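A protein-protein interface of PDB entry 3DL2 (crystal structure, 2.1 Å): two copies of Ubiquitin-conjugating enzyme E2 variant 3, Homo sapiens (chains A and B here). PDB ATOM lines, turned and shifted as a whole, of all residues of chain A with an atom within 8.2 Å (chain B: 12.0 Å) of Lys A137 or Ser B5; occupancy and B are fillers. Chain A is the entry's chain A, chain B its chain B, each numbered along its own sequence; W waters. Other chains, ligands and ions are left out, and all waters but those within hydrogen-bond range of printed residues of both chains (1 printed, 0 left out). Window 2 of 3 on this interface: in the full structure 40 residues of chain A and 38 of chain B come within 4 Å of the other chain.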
ATOM      1  N   VAL A 109       5.753  -8.368  -9.449  1.00  0.00           N
ATOM      2  CA  VAL A 109       4.661  -7.393  -9.452  1.00  0.00           C
ATOM      3  C   VAL A 109       3.252  -7.994  -9.600  1.00  0.00           C
ATOM      4  O   VAL A 109       2.343  -7.585  -8.870  1.00  0.00           O
ATOM      5  CB  VAL A 109       4.881  -6.261 -10.499  1.00  0.00           C
ATOM      6  CG1 VAL A 109       3.686  -5.304 -10.524  1.00  0.00           C
ATOM      7  CG2 VAL A 109       6.174  -5.490 -10.195  1.00  0.00           C
ATOM      8  N   PRO A 110       3.055  -8.943 -10.548  1.00  0.00           N
ATOM      9  CA  PRO A 110       1.692  -9.471 -10.708  1.00  0.00           C
ATOM     10  C   PRO A 110       1.178 -10.180  -9.452  1.00  0.00           C
ATOM     11  O   PRO A 110      -0.007 -10.073  -9.147  1.00  0.00           O
ATOM     12  CB  PRO A 110       1.822 -10.467 -11.872  1.00  0.00           C
ATOM     13  CG  PRO A 110       3.098 -10.066 -12.593  1.00  0.00           C
ATOM     14  CD  PRO A 110       3.999  -9.569 -11.501  1.00  0.00           C
ATOM     15  N   LEU A 121       1.344   1.175  -5.314  1.00  0.00           N
ATOM     16  CA  LEU A 121       2.650   0.613  -5.628  1.00  0.00           C
ATOM     17  C   LEU A 121       3.665   1.735  -5.739  1.00  0.00           C
ATOM     18  O   LEU A 121       3.513   2.638  -6.567  1.00  0.00           O
ATOM     19  CB  LEU A 121       2.582  -0.163  -6.945  1.00  0.00           C
ATOM     20  CG  LEU A 121       2.202  -1.656  -6.944  1.00  0.00           C
ATOM     21  CD1 LEU A 121       1.396  -2.124  -5.749  1.00  0.00           C
ATOM     22  CD2 LEU A 121       1.546  -2.069  -8.254  1.00  0.00           C
ATOM     23  N   ILE A 130      11.336   3.768 -16.263  1.00  0.00           N
ATOM     24  CA  ILE A 130      11.033   2.483 -16.892  1.00  0.00           C
ATOM     25  C   ILE A 130      10.469   1.482 -15.881  1.00  0.00           C
ATOM     26  O   ILE A 130       9.493   0.794 -16.176  1.00  0.00           O
ATOM     27  CB  ILE A 130      12.268   1.898 -17.610  1.00  0.00           C
ATOM     28  CG1 ILE A 130      12.540   2.678 -18.901  1.00  0.00           C
ATOM     29  CG2 ILE A 130      12.067   0.413 -17.930  1.00  0.00           C
ATOM     30  CD1 ILE A 130      13.997   2.805 -19.237  1.00  0.00           C
ATOM     31  N   MET A 131      11.065   1.407 -14.692  1.00  0.00           N
ATOM     32  CA  MET A 131      10.613   0.425 -13.701  1.00  0.00           C
ATOM     33  C   MET A 131       9.207   0.724 -13.200  1.00  0.00           C
ATOM     34  O   MET A 131       8.457  -0.211 -12.909  1.00  0.00           O
ATOM     35  CB  MET A 131      11.593   0.275 -12.531  1.00  0.00           C
ATOM     36  CG  MET A 131      12.994  -0.246 -12.913  1.00  0.00           C
ATOM     37  SD  MET A 131      13.021  -1.597 -14.127  1.00  0.00           S
ATOM     38  CE  MET A 131      12.237  -2.934 -13.237  1.00  0.00           C
ATOM     39  N   THR A 132       8.853   2.011 -13.107  1.00  0.00           N
ATOM     40  CA  THR A 132       7.487   2.410 -12.749  1.00  0.00           C
ATOM     41  C   THR A 132       6.485   2.032 -13.852  1.00  0.00           C
ATOM     42  O   THR A 132       5.410   1.486 -13.565  1.00  0.00           O
ATOM     43  CB  THR A 132       7.373   3.919 -12.390  1.00  0.00           C
ATOM     44  OG1 THR A 132       8.366   4.256 -11.414  1.00  0.00           O
ATOM     45  CG2 THR A 132       5.992   4.233 -11.792  1.00  0.00           C
ATOM     46  N   TYR A 133       6.842   2.305 -15.105  1.00  0.00           N
ATOM     47  CA  TYR A 133       6.023   1.896 -16.256  1.00  0.00           C
ATOM     48  C   TYR A 133       5.789   0.385 -16.257  1.00  0.00           C
ATOM     49  O   TYR A 133       4.664  -0.083 -16.423  1.00  0.00           O
ATOM     50  CB  TYR A 133       6.688   2.332 -17.566  1.00  0.00           C
ATOM     51  CG  TYR A 133       6.045   1.776 -18.823  1.00  0.00           C
ATOM     52  CD1 TYR A 133       5.046   2.488 -19.491  1.00  0.00           C
ATOM     53  CD2 TYR A 133       6.448   0.548 -19.352  1.00  0.00           C
ATOM     54  CE1 TYR A 133       4.454   1.985 -20.654  1.00  0.00           C
ATOM     55  CE2 TYR A 133       5.862   0.032 -20.513  1.00  0.00           C
ATOM     56  CZ  TYR A 133       4.870   0.755 -21.155  1.00  0.00           C
ATOM     57  OH  TYR A 133       4.296   0.255 -22.304  1.00  0.00           O
ATOM     58  N   VAL A 134       6.868  -0.368 -16.074  1.00  0.00           N
ATOM     59  CA  VAL A 134       6.812  -1.826 -16.040  1.00  0.00           C
ATOM     60  C   VAL A 134       5.882  -2.317 -14.916  1.00  0.00           C
ATOM     61  O   VAL A 134       5.073  -3.226 -15.114  1.00  0.00           O
ATOM     62  CB  VAL A 134       8.246  -2.412 -15.916  1.00  0.00           C
ATOM     63  CG1 VAL A 134       8.231  -3.822 -15.381  1.00  0.00           C
ATOM     64  CG2 VAL A 134       8.960  -2.359 -17.274  1.00  0.00           C
ATOM     65  N   THR A 135       5.992  -1.701 -13.745  1.00  0.00           N
ATOM     66  CA  THR A 135       5.153  -2.048 -12.602  1.00  0.00           C
ATOM     67  C   THR A 135       3.677  -1.756 -12.904  1.00  0.00           C
ATOM     68  O   THR A 135       2.790  -2.534 -12.541  1.00  0.00           O
ATOM     69  CB  THR A 135       5.632  -1.311 -11.330  1.00  0.00           C
ATOM     70  OG1 THR A 135       7.001  -1.661 -11.074  1.00  0.00           O
ATOM     71  CG2 THR A 135       4.781  -1.679 -10.110  1.00  0.00           C
ATOM     72  N   TRP A 136       3.432  -0.643 -13.592  1.00  0.00           N
ATOM     73  CA  TRP A 136       2.092  -0.277 -14.015  1.00  0.00           C
ATOM     74  C   TRP A 136       1.521  -1.318 -14.983  1.00  0.00           C
ATOM     75  O   TRP A 136       0.409  -1.805 -14.785  1.00  0.00           O
ATOM     76  CB  TRP A 136       2.099   1.130 -14.620  1.00  0.00           C
ATOM     77  CG  TRP A 136       0.780   1.597 -15.151  1.00  0.00           C
ATOM     78  CD1 TRP A 136      -0.398   1.700 -14.464  1.00  0.00           C
ATOM     79  CD2 TRP A 136       0.513   2.063 -16.480  1.00  0.00           C
ATOM     80  NE1 TRP A 136      -1.388   2.191 -15.290  1.00  0.00           N
ATOM     81  CE2 TRP A 136      -0.854   2.423 -16.532  1.00  0.00           C
ATOM     82  CE3 TRP A 136       1.297   2.215 -17.633  1.00  0.00           C
ATOM     83  CZ2 TRP A 136      -1.456   2.915 -17.694  1.00  0.00           C
ATOM     84  CZ3 TRP A 136       0.695   2.707 -18.790  1.00  0.00           C
ATOM     85  CH2 TRP A 136      -0.668   3.047 -18.809  1.00  0.00           C
ATOM     86  N   LYS A 137       2.296  -1.684 -16.002  1.00  0.00           N
ATOM     87  CA  LYS A 137       1.858  -2.690 -16.972  1.00  0.00           C
ATOM     88  C   LYS A 137       1.634  -4.078 -16.362  1.00  0.00           C
ATOM     89  O   LYS A 137       0.690  -4.765 -16.729  1.00  0.00           O
ATOM     90  CB  LYS A 137       2.840  -2.775 -18.144  1.00  0.00           C
ATOM     91  CG  LYS A 137       2.809  -1.551 -19.058  1.00  0.00           C
ATOM     92  CD  LYS A 137       1.584  -1.556 -19.976  1.00  0.00           C
ATOM     93  CE  LYS A 137       1.457  -0.250 -20.729  1.00  0.00           C
ATOM     94  NZ  LYS A 137       0.426  -0.335 -21.791  1.00  0.00           N
ATOM     95  N   LEU A 138       2.501  -4.484 -15.435  1.00  0.00           N
ATOM     96  CA  LEU A 138       2.427  -5.819 -14.832  1.00  0.00           C
ATOM     97  C   LEU A 138       1.322  -5.987 -13.779  1.00  0.00           C
ATOM     98  O   LEU A 138       0.843  -7.099 -13.552  1.00  0.00           O
ATOM     99  CB  LEU A 138       3.773  -6.210 -14.216  1.00  0.00           C
ATOM    100  CG  LEU A 138       4.934  -6.455 -15.184  1.00  0.00           C
ATOM    101  CD1 LEU A 138       6.237  -6.502 -14.402  1.00  0.00           C
ATOM    102  CD2 LEU A 138       4.725  -7.731 -15.994  1.00  0.00           C
ATOM    103  N   SER A 139       0.932  -4.893 -13.135  1.00  0.00           N
ATOM    104  CA  SER A 139      -0.039  -4.959 -12.045  1.00  0.00           C
ATOM    105  C   SER A 139      -1.497  -4.858 -12.481  1.00  0.00           C
ATOM    106  O   SER A 139      -2.380  -5.357 -11.774  1.00  0.00           O
ATOM    107  CB  SER A 139       0.248  -3.881 -11.009  1.00  0.00           C
ATOM    108  OG  SER A 139       0.169  -2.604 -11.604  1.00  0.00           O
ATOM    109  N   THR A 140      -1.745  -4.218 -13.628  1.00  0.00           N
ATOM    110  CA  THR A 140      -3.097  -3.872 -14.065  1.00  0.00           C
ATOM    111  C   THR A 140      -3.790  -2.978 -13.008  1.00  0.00           C
ATOM    112  O   THR A 140      -4.998  -3.098 -12.770  1.00  0.00           O
ATOM    113  CB  THR A 140      -3.948  -5.146 -14.417  1.00  0.00           C
ATOM    114  OG1 THR A 140      -3.165  -6.052 -15.212  1.00  0.00           O
ATOM    115  CG2 THR A 140      -5.206  -4.785 -15.185  1.00  0.00           C
ATOM    116  N   PHE A 141      -3.008  -2.100 -12.374  1.00  0.00           N
ATOM    117  CA  PHE A 141      -3.519  -1.074 -11.453  1.00  0.00           C
ATOM    118  C   PHE A 141      -3.805   0.203 -12.234  1.00  0.00           C
ATOM    119  O   PHE A 141      -3.200   0.421 -13.286  1.00  0.00           O
ATOM    120  CB  PHE A 141      -2.466  -0.731 -10.382  1.00  0.00           C
ATOM    121  CG  PHE A 141      -2.463  -1.648  -9.183  1.00  0.00           C
ATOM    122  CD1 PHE A 141      -2.936  -2.960  -9.269  1.00  0.00           C
ATOM    123  CD2 PHE A 141      -1.938  -1.201  -7.968  1.00  0.00           C
ATOM    124  CE1 PHE A 141      -2.912  -3.805  -8.157  1.00  0.00           C
ATOM    125  CE2 PHE A 141      -1.908  -2.037  -6.851  1.00  0.00           C
ATOM    126  CZ  PHE A 141      -2.400  -3.347  -6.950  1.00  0.00           C
ATOM    127  N   PRO A 142      -4.697   1.071 -11.710  1.00  0.00           N
ATOM    128  CA  PRO A 142      -4.864   2.382 -12.332  1.00  0.00           C
ATOM    129  C   PRO A 142      -3.597   3.220 -12.132  1.00  0.00           C
ATOM    130  O   PRO A 142      -2.889   3.039 -11.132  1.00  0.00           O
ATOM    131  CB  PRO A 142      -6.057   2.985 -11.580  1.00  0.00           C
ATOM    132  CG  PRO A 142      -6.099   2.269 -10.278  1.00  0.00           C
ATOM    133  CD  PRO A 142      -5.566   0.897 -10.528  1.00  0.00           C
ATOM    134  N   ALA A 143      -3.311   4.112 -13.077  1.00  0.00           N
ATOM    135  CA  ALA A 143      -2.050   4.863 -13.088  1.00  0.00           C
ATOM    136  C   ALA A 143      -1.821   5.703 -11.835  1.00  0.00           C
ATOM    137  O   ALA A 143      -0.673   5.931 -11.443  1.00  0.00           O
ATOM    138  CB  ALA A 143      -1.960   5.742 -14.332  1.00  0.00           C
ATOM    139  N   VAL A 146       0.140   3.786  -9.082  1.00  0.00           N
ATOM    140  CA  VAL A 146       1.489   3.318  -9.390  1.00  0.00           C
ATOM    141  C   VAL A 146       2.409   4.522  -9.574  1.00  0.00           C
ATOM    142  O   VAL A 146       2.302   5.257 -10.554  1.00  0.00           O
ATOM    143  CB  VAL A 146       1.555   2.398 -10.652  1.00  0.00           C
ATOM    144  CG1 VAL A 146       2.942   1.778 -10.792  1.00  0.00           C
ATOM    145  CG2 VAL A 146       0.520   1.282 -10.584  1.00  0.00           C
ATOM    146  N   LEU A 246       2.452   8.931 -14.628  1.00  0.00           N
ATOM    147  CA  LEU A 246       2.106   8.860 -16.053  1.00  0.00           C
ATOM    148  C   LEU A 246       2.029  10.266 -16.656  1.00  0.00           C
ATOM    149  O   LEU A 246       1.198  11.078 -16.251  1.00  0.00           O
ATOM    150  CB  LEU A 246       0.805   8.081 -16.267  1.00  0.00           C
ATOM    151  CG  LEU A 246       0.379   7.769 -17.709  1.00  0.00           C
ATOM    152  CD1 LEU A 246       1.439   6.980 -18.463  1.00  0.00           C
ATOM    153  CD2 LEU A 246      -0.950   7.025 -17.724  1.00  0.00           C
ATOM    154  N   GLU A 256       3.171   6.842 -23.513  1.00  0.00           N
ATOM    155  CA  GLU A 256       3.000   6.364 -22.142  1.00  0.00           C
ATOM    156  C   GLU A 256       4.347   6.214 -21.438  1.00  0.00           C
ATOM    157  O   GLU A 256       5.006   5.171 -21.518  1.00  0.00           O
ATOM    158  CB  GLU A 256       2.185   5.066 -22.106  1.00  0.00           C
ATOM    159  CG  GLU A 256       0.732   5.277 -22.502  1.00  0.00           C
ATOM    160  CD  GLU A 256      -0.098   4.006 -22.484  1.00  0.00           C
ATOM    161  OE1 GLU A 256       0.476   2.896 -22.473  1.00  0.00           O
ATOM    162  OE2 GLU A 256      -1.338   4.126 -22.492  1.00  0.00           O
ATOM    163  N   PHE A 258       6.491   7.464 -17.653  1.00  0.00           N
ATOM    164  CA  PHE A 258       6.421   8.050 -16.330  1.00  0.00           C
ATOM    165  C   PHE A 258       7.601   9.002 -16.160  1.00  0.00           C
ATOM    166  O   PHE A 258       8.747   8.618 -16.352  1.00  0.00           O
ATOM    167  CB  PHE A 258       6.392   6.957 -15.248  1.00  0.00           C
ATOM    168  CG  PHE A 258       5.104   6.157 -15.226  1.00  0.00           C
ATOM    169  CD1 PHE A 258       4.718   5.388 -16.324  1.00  0.00           C
ATOM    170  CD2 PHE A 258       4.284   6.172 -14.107  1.00  0.00           C
ATOM    171  CE1 PHE A 258       3.529   4.654 -16.305  1.00  0.00           C
ATOM    172  CE2 PHE A 258       3.098   5.443 -14.075  1.00  0.00           C
ATOM    173  CZ  PHE A 258       2.719   4.686 -15.172  1.00  0.00           C
ATOM    174  N   GLN A 298      11.699   1.467 -23.807  1.00  0.00           N
ATOM    175  CA  GLN A 298      10.543   0.632 -23.456  1.00  0.00           C
ATOM    176  C   GLN A 298      10.090  -0.249 -24.624  1.00  0.00           C
ATOM    177  O   GLN A 298       9.695  -1.398 -24.418  1.00  0.00           O
ATOM    178  CB  GLN A 298       9.380   1.497 -22.966  1.00  0.00           C
ATOM    179  CG  GLN A 298       9.589   2.052 -21.564  1.00  0.00           C
ATOM    180  CD  GLN A 298       8.498   3.011 -21.125  1.00  0.00           C
ATOM    181  OE1 GLN A 298       7.524   3.261 -21.848  1.00  0.00           O
ATOM    182  NE2 GLN A 298       8.657   3.555 -19.934  1.00  0.00           N
ATOM    183  N   LEU A 303       8.297  -7.294 -22.253  1.00  0.00           N
ATOM    184  CA  LEU A 303       7.440  -7.065 -21.087  1.00  0.00           C
ATOM    185  C   LEU A 303       6.351  -8.122 -20.908  1.00  0.00           C
ATOM    186  O   LEU A 303       6.042  -8.892 -21.816  1.00  0.00           O
ATOM    187  CB  LEU A 303       6.790  -5.678 -21.151  1.00  0.00           C
ATOM    188  CG  LEU A 303       7.486  -4.539 -20.404  1.00  0.00           C
ATOM    189  CD1 LEU A 303       8.421  -3.777 -21.328  1.00  0.00           C
ATOM    190  CD2 LEU A 303       6.444  -3.601 -19.810  1.00  0.00           C
ATOM    191  OXT LEU A 303       5.742  -8.207 -19.839  1.00  0.00           O
ATOM    192  N   GLY B   1      -4.050   9.092 -15.519  1.00  0.00           N
ATOM    193  CA  GLY B   1      -4.398   8.993 -14.074  1.00  0.00           C
ATOM    194  C   GLY B   1      -5.251   7.779 -13.762  1.00  0.00           C
ATOM    195  O   GLY B   1      -4.868   6.931 -12.958  1.00  0.00           O
ATOM    196  N   SER B   2      -6.413   7.700 -14.403  1.00  0.00           N
ATOM    197  CA  SER B   2      -7.335   6.581 -14.208  1.00  0.00           C
ATOM    198  C   SER B   2      -6.855   5.311 -14.910  1.00  0.00           C
ATOM    199  O   SER B   2      -7.103   4.202 -14.434  1.00  0.00           O
ATOM    200  CB  SER B   2      -8.734   6.947 -14.724  1.00  0.00           C
ATOM    201  OG  SER B   2      -9.214   8.147 -14.139  1.00  0.00           O
ATOM    202  N   SER B   3      -6.153   5.492 -16.029  1.00  0.00           N
ATOM    203  CA  SER B   3      -5.901   4.426 -17.007  1.00  0.00           C
ATOM    204  C   SER B   3      -5.174   3.199 -16.461  1.00  0.00           C
ATOM    205  O   SER B   3      -4.284   3.313 -15.618  1.00  0.00           O
ATOM    206  CB  SER B   3      -5.155   4.983 -18.225  1.00  0.00           C
ATOM    207  OG  SER B   3      -5.180   4.063 -19.305  1.00  0.00           O
ATOM    208  N   LYS B   4      -5.572   2.032 -16.963  1.00  0.00           N
ATOM    209  CA  LYS B   4      -4.933   0.763 -16.626  1.00  0.00           C
ATOM    210  C   LYS B   4      -4.292   0.163 -17.877  1.00  0.00           C
ATOM    211  O   LYS B   4      -4.972  -0.048 -18.882  1.00  0.00           O
ATOM    212  CB  LYS B   4      -5.945  -0.221 -16.026  1.00  0.00           C
ATOM    213  CG  LYS B   4      -6.777   0.336 -14.877  1.00  0.00           C
ATOM    214  CD  LYS B   4      -7.089  -0.743 -13.856  1.00  0.00           C
ATOM    215  CE  LYS B   4      -8.116  -0.278 -12.838  1.00  0.00           C
ATOM    216  NZ  LYS B   4      -8.160  -1.189 -11.661  1.00  0.00           N
ATOM    217  N   SER B   5      -2.987  -0.103 -17.796  1.00  0.00           N
ATOM    218  CA  SER B   5      -2.180  -0.631 -18.910  1.00  0.00           C
ATOM    219  C   SER B   5      -2.377   0.130 -20.230  1.00  0.00           C
ATOM    220  O   SER B   5      -3.119  -0.301 -21.121  1.00  0.00           O
ATOM    221  CB  SER B   5      -2.392  -2.143 -19.091  1.00  0.00           C
ATOM    222  OG  SER B   5      -3.680  -2.434 -19.611  1.00  0.00           O
HETATM  223  O   HOH W   1      -2.015  -1.117 -15.548  1.00  0.00           O
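Water W1 lies within hydrogen-bond range of O of Trp A136 (2.6 Å), N of Ser B5 (2.7 Å) and O of Phe A141 (3.0 Å).
Among the printed residues, pairs that only touch across the chains: Lys A137 with Ser B5 (3.2 Å), Pro A142 with Ser B2 (3.3 Å), Thr A140 with Lys B4 (3.3 Å), Trp A136 with Ser B5 (3.4 Å), Pro A142 with Ser B3 (3.5 Å), Pro A142 with Lys B4 (3.5 Å), Phe A141 with Lys B4 (3.8 Å), Phe A141 with Ser B3 (3.9 Å) and Trp A136 with Lys B4 (3.96 Å).
The backbone carbonyl oxygen (O) of Phe A141 is in hydrogen-bond range of the indole nitrogen (NE1) of Trp A136 (3.2 Å).
The side-chain hydroxyl of Ser A139 sits at hydrogen-bond distance from the backbone carbonyl oxygen of Trp A136.
The side-chain hydroxyl (OG) of Ser A139 sits close to the backbone NH (N) of Phe A141, 3.3 Å away.
The side-chain amino group (NZ) of Lys A137 is in salt-bridge range of the side-chain carboxylate (OE1) of Glu A256 (3.3 Å).
The backbone NH of Ala A143 lies within hydrogen-bond range of the backbone carbonyl oxygen of Gly B1 (3.2 Å).
The indole nitrogen (NE1) of Trp A136 is in hydrogen-bond range of the backbone carbonyl oxygen (O) of Ser B3 (3.1 Å).
The backbone NH (N) of Ala A143 sits at hydrogen-bond distance from the backbone carbonyl oxygen (O) of Ser B3 (2.8 Å).
Printed residues of chain B that touch a printed residue of chain A: Gly B1, Ser B2, Ser B3, Lys B4 and Ser B5.
Among the printed residues, 12 pairs touch across the chains.
Among the printed residues, no Asp or Glu carboxylate lies within 4 Å of a Lys or Arg side-chain nitrogen of the other chain.
Of chain B, only Ser B5 (3.2 Å) comes within 4 Å of Lys A137.
Ser B5 touches just these residues of chain A: Trp A136 (3.4 Å) and Lys A137 (3.2 Å).
No residue of chain B comes within 4 Å of Thr A135.
Of chain B, only Ser B3 (3.1 Å), Lys B4 (3.96 Å) and Ser B5 (3.4 Å) come within 4 Å of Trp A136.
No residue of chain B comes within 4 Å of Ser A139.
Of chain B, only Lys B4 (3.3 Å) comes within 4 Å of Thr A140.
Of the printed residues of chain B, Pro A142 touches Ser B2, Ser B3 and Lys B4.
Printed residues of chain B within 4 Å of Phe A141: Ser B3 and Lys B4.
Of the printed residues of chain B, Ala A143 touches Gly B1 and Ser B3.
Of the printed residues of chain A, Gly B1 touches Ala A143 (3.2 Å).
Printed residues of chain A within 4 Å of Lys B4: Trp A136 (3.96 Å), Thr A140 (3.3 Å), Phe A141 (3.8 Å) and Pro A142 (3.5 Å).
No position is printed for both chains.
Of the 12 pairs that touch across the chains among the printed residues, none has its exchanged pair printed and touching as well.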
